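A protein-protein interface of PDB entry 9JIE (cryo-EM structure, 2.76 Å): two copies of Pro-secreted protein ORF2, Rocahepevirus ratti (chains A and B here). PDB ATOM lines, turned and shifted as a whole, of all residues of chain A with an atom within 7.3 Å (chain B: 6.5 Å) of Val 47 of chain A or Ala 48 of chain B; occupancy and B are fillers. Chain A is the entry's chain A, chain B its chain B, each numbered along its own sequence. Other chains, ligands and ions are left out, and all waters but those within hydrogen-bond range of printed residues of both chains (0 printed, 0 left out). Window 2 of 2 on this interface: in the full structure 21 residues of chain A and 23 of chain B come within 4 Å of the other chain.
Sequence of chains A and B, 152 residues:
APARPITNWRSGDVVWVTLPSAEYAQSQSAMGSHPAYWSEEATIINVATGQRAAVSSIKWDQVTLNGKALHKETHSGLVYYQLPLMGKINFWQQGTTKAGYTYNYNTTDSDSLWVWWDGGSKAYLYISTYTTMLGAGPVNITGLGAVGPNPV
Val 14 of chain A touches its own counterpart, Val 14 of chain B.
Val 14 of chain A touches Val 47 of chain B, and with the chains exchanged Val 47 of chain A touches Val 14 of chain B.
Val 47 of chain B touches its own counterpart, Val 47 of chain A.
Val 47 of chain A touches Ala 48 of chain B, and with the chains exchanged Ala 48 of chain A touches Val 47 of chain B.
Of the 9 pairs that touch across the chains among the printed residues, 6 have their exchanged pair printed and touching as well.
Val 47 of chain A touches three residues of chain B.
Ala 48 of chain B touches one residue of chain A.
Printed residues of chain B within 4 Å of Val 14 of chain A: Val 14 (3.9 Å) and Val 47 (3.9 Å).
Printed residues of chain A within 4 Å of Gly 12 of chain B: Trp 16.
The nearest residue of chain B that does not touch Val 47 of chain A is Thr 49 of chain B (5.9 Å).
The nearest printed residue of chain A that does not touch Gly 12 of chain B is Leu 144 of chain A (6.6 Å).
The backbone carbonyl oxygen (O) of Val 14 of chain A lies close to the side-chain amide oxygen (OD1) of Asn 46 of chain A, 3.2 Å away.
O of Val 14 of chain A is in hydrogen-bond range of N of Val 47 of chain A.
The backbone carbonyl oxygen of Trp 16 of chain A is in hydrogen-bond range of the backbone NH of Ile 45 of chain A (2.7 Å).
OD1 of Asn 46 of chain A sits at hydrogen-bond distance from N of Ala 48 of chain A, at 3.1 Å.
O of Val 14 of chain B lies close to OD1 of Asn 46 of chain B (2.6 Å).
The backbone NH (N) of Val 47 of chain B is in hydrogen-bond range of the backbone carbonyl oxygen (O) of Val 14 of chain B (2.8 Å).
CG1 of Val 14 of chain A touches CG1 of Val 14 of chain B (3.9 Å).
CB of Val 14 of chain A touches CG1 of Val 47 of chain B (3.9 Å).
CH2 of Trp 16 of chain A touches O of Gly 12 of chain B, at 3.2 Å.
CG2 of Val 14 of chain B touches CZ3 of Trp 16 of chain A, at 3.3 Å.
Val 47 of chain A touches Val 14 of chain B (CG1 to CB, 3.9 Å).
Val 47 of chain A touches Val 47 of chain B.
CG1 of Val 47 of chain A touches N of Ala 48 of chain B, at 3.98 Å.
CA of Ala 48 of chain A touches CG1 of Val 47 of chain B (3.9 Å).
Leu 144 of chain A touches Val 14 of chain B.
Of the 11 printed residues of chain B, 4 touch a printed residue of chain A.
Among the printed residues, 9 pairs touch across the chains.
Among the printed residues, no Asp or Glu carboxylate lies within 4 Å of a Lys or Arg side-chain nitrogen of the other chain.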
ATOM      1  N   ARG A   4      20.862 -12.745  -7.415  1.00  0.00           N
ATOM      2  CA  ARG A   4      19.658 -13.511  -7.132  1.00  0.00           C
ATOM      3  C   ARG A   4      19.811 -14.256  -5.809  1.00  0.00           C
ATOM      4  O   ARG A   4      20.846 -14.897  -5.580  1.00  0.00           O
ATOM      5  CB  ARG A   4      19.378 -14.499  -8.262  1.00  0.00           C
ATOM      6  CG  ARG A   4      18.112 -15.306  -8.071  1.00  0.00           C
ATOM      7  CD  ARG A   4      17.912 -16.301  -9.193  1.00  0.00           C
ATOM      8  NE  ARG A   4      18.957 -17.315  -9.206  1.00  0.00           N
ATOM      9  CZ  ARG A   4      19.234 -18.089 -10.245  1.00  0.00           C
ATOM     10  NH1 ARG A   4      18.551 -18.000 -11.373  1.00  0.00           N
ATOM     11  NH2 ARG A   4      20.222 -18.972 -10.151  1.00  0.00           N
ATOM     12  N   TRP A   9      15.353 -20.624  -7.214  1.00  0.00           N
ATOM     13  CA  TRP A   9      15.987 -21.649  -8.026  1.00  0.00           C
ATOM     14  C   TRP A   9      15.234 -21.796  -9.339  1.00  0.00           C
ATOM     15  O   TRP A   9      14.003 -21.728  -9.369  1.00  0.00           O
ATOM     16  CB  TRP A   9      16.030 -22.993  -7.295  1.00  0.00           C
ATOM     17  CG  TRP A   9      17.073 -23.061  -6.222  1.00  0.00           C
ATOM     18  CD1 TRP A   9      16.876 -22.931  -4.878  1.00  0.00           C
ATOM     19  CD2 TRP A   9      18.478 -23.275  -6.403  1.00  0.00           C
ATOM     20  NE1 TRP A   9      18.071 -23.051  -4.211  1.00  0.00           N
ATOM     21  CE2 TRP A   9      19.070 -23.263  -5.125  1.00  0.00           C
ATOM     22  CE3 TRP A   9      19.293 -23.474  -7.521  1.00  0.00           C
ATOM     23  CZ2 TRP A   9      20.437 -23.443  -4.935  1.00  0.00           C
ATOM     24  CZ3 TRP A   9      20.649 -23.653  -7.330  1.00  0.00           C
ATOM     25  CH2 TRP A   9      21.207 -23.637  -6.049  1.00  0.00           C
ATOM     26  N   ASP A  13      19.775 -24.709 -13.261  1.00  0.00           N
ATOM     27  CA  ASP A  13      20.796 -24.105 -12.420  1.00  0.00           C
ATOM     28  C   ASP A  13      21.692 -25.182 -11.822  1.00  0.00           C
ATOM     29  O   ASP A  13      21.243 -26.291 -11.527  1.00  0.00           O
ATOM     30  CB  ASP A  13      20.153 -23.282 -11.307  1.00  0.00           C
ATOM     31  CG  ASP A  13      19.774 -21.888 -11.758  1.00  0.00           C
ATOM     32  OD1 ASP A  13      20.287 -21.441 -12.805  1.00  0.00           O
ATOM     33  OD2 ASP A  13      18.965 -21.239 -11.064  1.00  0.00           O
ATOM     34  N   VAL A  14      22.964 -24.850 -11.638  1.00  0.00           N
ATOM     35  CA  VAL A  14      23.933 -25.782 -11.075  1.00  0.00           C
ATOM     36  C   VAL A  14      24.043 -25.524  -9.579  1.00  0.00           C
ATOM     37  O   VAL A  14      24.303 -24.394  -9.150  1.00  0.00           O
ATOM     38  CB  VAL A  14      25.299 -25.651 -11.764  1.00  0.00           C
ATOM     39  CG1 VAL A  14      26.378 -26.294 -10.914  1.00  0.00           C
ATOM     40  CG2 VAL A  14      25.253 -26.300 -13.128  1.00  0.00           C
ATOM     41  N   VAL A  15      23.778 -26.519  -8.719  1.00  0.00           N
ATOM     42  CA  VAL A  15      23.823 -26.511  -7.239  1.00  0.00           C
ATOM     43  C   VAL A  15      25.164 -27.128  -6.810  1.00  0.00           C
ATOM     44  O   VAL A  15      25.691 -28.056  -7.424  1.00  0.00           O
ATOM     45  CB  VAL A  15      22.632 -27.221  -6.576  1.00  0.00           C
ATOM     46  CG1 VAL A  15      22.491 -28.673  -6.955  1.00  0.00           C
ATOM     47  CG2 VAL A  15      22.695 -27.083  -5.073  1.00  0.00           C
ATOM     48  N   TRP A  16      25.772 -26.607  -5.751  1.00  0.00           N
ATOM     49  CA  TRP A  16      27.038 -27.145  -5.285  1.00  0.00           C
ATOM     50  C   TRP A  16      26.941 -27.343  -3.816  1.00  0.00           C
ATOM     51  O   TRP A  16      27.055 -26.454  -3.137  1.00  0.00           O
ATOM     52  CB  TRP A  16      28.218 -26.264  -5.661  1.00  0.00           C
ATOM     53  CG  TRP A  16      29.539 -26.882  -5.266  1.00  0.00           C
ATOM     54  CD1 TRP A  16      29.930 -27.274  -4.019  1.00  0.00           C
ATOM     55  CD2 TRP A  16      30.614 -27.262  -6.148  1.00  0.00           C
ATOM     56  NE1 TRP A  16      31.165 -27.848  -4.060  1.00  0.00           N
ATOM     57  CE2 TRP A  16      31.609 -27.855  -5.350  1.00  0.00           C
ATOM     58  CE3 TRP A  16      30.834 -27.157  -7.521  1.00  0.00           C
ATOM     59  CZ2 TRP A  16      32.802 -28.333  -5.881  1.00  0.00           C
ATOM     60  CZ3 TRP A  16      32.009 -27.643  -8.047  1.00  0.00           C
ATOM     61  CH2 TRP A  16      32.975 -28.226  -7.239  1.00  0.00           C
ATOM     62  N   VAL A  17      26.960 -28.564  -3.381  1.00  0.00           N
ATOM     63  CA  VAL A  17      26.801 -28.927  -1.990  1.00  0.00           C
ATOM     64  C   VAL A  17      28.103 -29.219  -1.319  1.00  0.00           C
ATOM     65  O   VAL A  17      28.963 -29.743  -1.889  1.00  0.00           O
ATOM     66  CB  VAL A  17      25.946 -30.178  -1.783  1.00  0.00           C
ATOM     67  CG1 VAL A  17      24.476 -29.885  -2.004  1.00  0.00           C
ATOM     68  CG2 VAL A  17      26.325 -31.357  -2.627  1.00  0.00           C
ATOM     69  N   ILE A  45      25.640 -24.258  -2.423  1.00  0.00           N
ATOM     70  CA  ILE A  45      26.208 -23.240  -3.299  1.00  0.00           C
ATOM     71  C   ILE A  45      25.517 -23.323  -4.652  1.00  0.00           C
ATOM     72  O   ILE A  45      25.322 -24.418  -5.194  1.00  0.00           O
ATOM     73  CB  ILE A  45      27.736 -23.405  -3.470  1.00  0.00           C
ATOM     74  CG1 ILE A  45      28.450 -23.427  -2.116  1.00  0.00           C
ATOM     75  CG2 ILE A  45      28.297 -22.298  -4.344  1.00  0.00           C
ATOM     76  CD1 ILE A  45      28.565 -24.797  -1.497  1.00  0.00           C
ATOM     77  N   ASN A  46      25.138 -22.162  -5.193  1.00  0.00           N
ATOM     78  CA  ASN A  46      24.641 -22.054  -6.561  1.00  0.00           C
ATOM     79  C   ASN A  46      25.806 -21.604  -7.436  1.00  0.00           C
ATOM     80  O   ASN A  46      26.309 -20.487  -7.284  1.00  0.00           O
ATOM     81  CB  ASN A  46      23.471 -21.078  -6.648  1.00  0.00           C
ATOM     82  CG  ASN A  46      22.837 -21.049  -8.024  1.00  0.00           C
ATOM     83  OD1 ASN A  46      23.492 -21.324  -9.026  1.00  0.00           O
ATOM     84  ND2 ASN A  46      21.553 -20.715  -8.078  1.00  0.00           N
ATOM     85  N   VAL A  47      26.239 -22.480  -8.343  1.00  0.00           N
ATOM     86  CA  VAL A  47      27.466 -22.230  -9.092  1.00  0.00           C
ATOM     87  C   VAL A  47      27.280 -21.093 -10.089  1.00  0.00           C
ATOM     88  O   VAL A  47      28.185 -20.275 -10.291  1.00  0.00           O
ATOM     89  CB  VAL A  47      27.937 -23.518  -9.785  1.00  0.00           C
ATOM     90  CG1 VAL A  47      29.194 -23.252 -10.588  1.00  0.00           C
ATOM     91  CG2 VAL A  47      28.176 -24.610  -8.759  1.00  0.00           C
ATOM     92  N   ALA A  48      26.111 -21.023 -10.730  1.00  0.00           N
ATOM     93  CA  ALA A  48      25.917 -20.077 -11.825  1.00  0.00           C
ATOM     94  C   ALA A  48      26.099 -18.637 -11.362  1.00  0.00           C
ATOM     95  O   ALA A  48      26.763 -17.838 -12.030  1.00  0.00           O
ATOM     96  CB  ALA A  48      24.533 -20.271 -12.444  1.00  0.00           C
ATOM     97  N   THR A  49      25.517 -18.287 -10.216  1.00  0.00           N
ATOM     98  CA  THR A  49      25.606 -16.932  -9.688  1.00  0.00           C
ATOM     99  C   THR A  49      26.547 -16.805  -8.497  1.00  0.00           C
ATOM    100  O   THR A  49      26.798 -15.684  -8.046  1.00  0.00           O
ATOM    101  CB  THR A  49      24.215 -16.423  -9.293  1.00  0.00           C
ATOM    102  OG1 THR A  49      23.768 -17.120  -8.126  1.00  0.00           O
ATOM    103  CG2 THR A  49      23.224 -16.654 -10.424  1.00  0.00           C
ATOM    104  N   GLY A  50      27.070 -17.915  -7.980  1.00  0.00           N
ATOM    105  CA  GLY A  50      28.035 -17.878  -6.902  1.00  0.00           C
ATOM    106  C   GLY A  50      27.457 -17.751  -5.510  1.00  0.00           C
ATOM    107  O   GLY A  50      28.229 -17.690  -4.545  1.00  0.00           O
ATOM    108  N   GLN A  51      26.135 -17.707  -5.368  1.00  0.00           N
ATOM    109  CA  GLN A  51      25.531 -17.564  -4.052  1.00  0.00           C
ATOM    110  C   GLN A  51      25.666 -18.855  -3.256  1.00  0.00           C
ATOM    111  O   GLN A  51      25.540 -19.955  -3.800  1.00  0.00           O
ATOM    112  CB  GLN A  51      24.060 -17.177  -4.182  1.00  0.00           C
ATOM    113  CG  GLN A  51      23.824 -16.019  -5.122  1.00  0.00           C
ATOM    114  CD  GLN A  51      24.609 -14.789  -4.728  1.00  0.00           C
ATOM    115  OE1 GLN A  51      25.278 -14.173  -5.555  1.00  0.00           O
ATOM    116  NE2 GLN A  51      24.529 -14.419  -3.455  1.00  0.00           N
ATOM    117  N   GLY A 143      29.429 -32.338  -3.367  1.00  0.00           N
ATOM    118  CA  GLY A 143      28.433 -32.692  -4.378  1.00  0.00           C
ATOM    119  C   GLY A 143      28.108 -31.675  -5.400  1.00  0.00           C
ATOM    120  O   GLY A 143      28.522 -30.560  -5.246  1.00  0.00           O
ATOM    121  N   LEU A 144      27.438 -32.145  -6.449  1.00  0.00           N
ATOM    122  CA  LEU A 144      27.156 -31.257  -7.568  1.00  0.00           C
ATOM    123  C   LEU A 144      25.949 -31.779  -8.336  1.00  0.00           C
ATOM    124  O   LEU A 144      25.801 -32.989  -8.518  1.00  0.00           O
ATOM    125  CB  LEU A 144      28.369 -31.146  -8.500  1.00  0.00           C
ATOM    126  CG  LEU A 144      28.246 -30.225  -9.714  1.00  0.00           C
ATOM    127  CD1 LEU A 144      28.563 -28.796  -9.322  1.00  0.00           C
ATOM    128  CD2 LEU A 144      29.161 -30.695 -10.829  1.00  0.00           C
ATOM    129  N   GLY A 145      25.100 -30.858  -8.794  1.00  0.00           N
ATOM    130  CA  GLY A 145      23.925 -31.225  -9.565  1.00  0.00           C
ATOM    131  C   GLY A 145      23.380 -30.042 -10.333  1.00  0.00           C
ATOM    132  O   GLY A 145      23.827 -28.905 -10.170  1.00  0.00           O
ATOM    133  N   ARG B   4      38.005 -15.075 -17.644  1.00  0.00           N
ATOM    134  CA  ARG B   4      38.969 -16.140 -17.876  1.00  0.00           C
ATOM    135  C   ARG B   4      38.581 -16.927 -19.124  1.00  0.00           C
ATOM    136  O   ARG B   4      37.409 -17.297 -19.278  1.00  0.00           O
ATOM    137  CB  ARG B   4      39.030 -17.069 -16.665  1.00  0.00           C
ATOM    138  CG  ARG B   4      39.407 -18.497 -17.005  1.00  0.00           C
ATOM    139  CD  ARG B   4      40.014 -19.209 -15.817  1.00  0.00           C
ATOM    140  NE  ARG B   4      38.998 -19.610 -14.853  1.00  0.00           N
ATOM    141  CZ  ARG B   4      39.000 -20.764 -14.203  1.00  0.00           C
ATOM    142  NH1 ARG B   4      39.949 -21.664 -14.398  1.00  0.00           N
ATOM    143  NH2 ARG B   4      38.027 -21.022 -13.336  1.00  0.00           N
ATOM    144  N   GLY B  12      38.058 -28.255  -9.572  1.00  0.00           N
ATOM    145  CA  GLY B  12      36.847 -27.831  -8.908  1.00  0.00           C
ATOM    146  C   GLY B  12      35.935 -26.957  -9.739  1.00  0.00           C
ATOM    147  O   GLY B  12      34.829 -26.638  -9.285  1.00  0.00           O
ATOM    148  N   ASP B  13      36.358 -26.552 -10.932  1.00  0.00           N
ATOM    149  CA  ASP B  13      35.493 -25.773 -11.805  1.00  0.00           C
ATOM    150  C   ASP B  13      34.377 -26.648 -12.361  1.00  0.00           C
ATOM    151  O   ASP B  13      34.575 -27.831 -12.646  1.00  0.00           O
ATOM    152  CB  ASP B  13      36.299 -25.165 -12.950  1.00  0.00           C
ATOM    153  CG  ASP B  13      36.975 -23.870 -12.559  1.00  0.00           C
ATOM    154  OD1 ASP B  13      36.584 -23.280 -11.530  1.00  0.00           O
ATOM    155  OD2 ASP B  13      37.896 -23.438 -13.282  1.00  0.00           O
ATOM    156  N   VAL B  14      33.204 -26.059 -12.515  1.00  0.00           N
ATOM    157  CA  VAL B  14      32.046 -26.776 -13.034  1.00  0.00           C
ATOM    158  C   VAL B  14      31.987 -26.579 -14.542  1.00  0.00           C
ATOM    159  O   VAL B  14      31.990 -25.444 -15.031  1.00  0.00           O
ATOM    160  CB  VAL B  14      30.749 -26.301 -12.362  1.00  0.00           C
ATOM    161  CG1 VAL B  14      29.549 -26.763 -13.159  1.00  0.00           C
ATOM    162  CG2 VAL B  14      30.673 -26.835 -10.948  1.00  0.00           C
ATOM    163  N   VAL B  15      31.929 -27.685 -15.283  1.00  0.00           N
ATOM    164  CA  VAL B  15      31.885 -27.672 -16.739  1.00  0.00           C
ATOM    165  C   VAL B  15      30.512 -28.154 -17.191  1.00  0.00           C
ATOM    166  O   VAL B  15      29.913 -29.081 -16.646  1.00  0.00           O
ATOM    167  CB  VAL B  15      33.016 -28.524 -17.347  1.00  0.00           C
ATOM    168  CG1 VAL B  15      32.928 -29.975 -16.895  1.00  0.00           C
ATOM    169  CG2 VAL B  15      32.987 -28.439 -18.861  1.00  0.00           C
ATOM    170  N   ASN B  46      31.623 -23.432 -19.208  1.00  0.00           N
ATOM    171  CA  ASN B  46      32.123 -23.363 -17.838  1.00  0.00           C
ATOM    172  C   ASN B  46      31.105 -22.580 -17.018  1.00  0.00           C
ATOM    173  O   ASN B  46      30.879 -21.392 -17.267  1.00  0.00           O
ATOM    174  CB  ASN B  46      33.499 -22.706 -17.785  1.00  0.00           C
ATOM    175  CG  ASN B  46      34.172 -22.874 -16.438  1.00  0.00           C
ATOM    176  OD1 ASN B  46      33.963 -23.870 -15.750  1.00  0.00           O
ATOM    177  ND2 ASN B  46      34.983 -21.897 -16.055  1.00  0.00           N
ATOM    178  N   VAL B  47      30.487 -23.249 -16.043  1.00  0.00           N
ATOM    179  CA  VAL B  47      29.371 -22.648 -15.319  1.00  0.00           C
ATOM    180  C   VAL B  47      29.850 -21.524 -14.408  1.00  0.00           C
ATOM    181  O   VAL B  47      29.179 -20.495 -14.270  1.00  0.00           O
ATOM    182  CB  VAL B  47      28.608 -23.725 -14.531  1.00  0.00           C
ATOM    183  CG1 VAL B  47      27.465 -23.097 -13.760  1.00  0.00           C
ATOM    184  CG2 VAL B  47      28.095 -24.798 -15.470  1.00  0.00           C
ATOM    185  N   ALA B  48      31.009 -21.701 -13.770  1.00  0.00           N
ATOM    186  CA  ALA B  48      31.446 -20.758 -12.743  1.00  0.00           C
ATOM    187  C   ALA B  48      31.614 -19.354 -13.308  1.00  0.00           C
ATOM    188  O   ALA B  48      31.182 -18.371 -12.695  1.00  0.00           O
ATOM    189  CB  ALA B  48      32.748 -21.243 -12.109  1.00  0.00           C
ATOM    190  N   THR B  49      32.239 -19.238 -14.478  1.00  0.00           N
ATOM    191  CA  THR B  49      32.460 -17.942 -15.106  1.00  0.00           C
ATOM    192  C   THR B  49      31.549 -17.684 -16.299  1.00  0.00           C
ATOM    193  O   THR B  49      31.558 -16.570 -16.834  1.00  0.00           O
ATOM    194  CB  THR B  49      33.923 -17.809 -15.546  1.00  0.00           C
ATOM    195  OG1 THR B  49      34.166 -18.670 -16.665  1.00  0.00           O
ATOM    196  CG2 THR B  49      34.858 -18.192 -14.410  1.00  0.00           C
ATOM    197  N   GLY B  50      30.769 -18.674 -16.729  1.00  0.00           N
ATOM    198  CA  GLY B  50      29.824 -18.491 -17.809  1.00  0.00           C
ATOM    199  C   GLY B  50      30.397 -18.610 -19.204  1.00  0.00           C
ATOM    200  O   GLY B  50      29.644 -18.467 -20.176  1.00  0.00           O
ATOM    201  N   GLN B  51      31.696 -18.862 -19.342  1.00  0.00           N
ATOM    202  CA  GLN B  51      32.306 -18.938 -20.660  1.00  0.00           C
ATOM    203  C   GLN B  51      31.895 -20.218 -21.374  1.00  0.00           C
ATOM    204  O   GLN B  51      31.796 -21.286 -20.765  1.00  0.00           O
ATOM    205  CB  GLN B  51      33.826 -18.863 -20.548  1.00  0.00           C
ATOM    206  CG  GLN B  51      34.311 -17.702 -19.712  1.00  0.00           C
ATOM    207  CD  GLN B  51      33.828 -16.370 -20.240  1.00  0.00           C
ATOM    208  OE1 GLN B  51      33.318 -15.541 -19.490  1.00  0.00           O
ATOM    209  NE2 GLN B  51      33.988 -16.157 -21.541  1.00  0.00           N
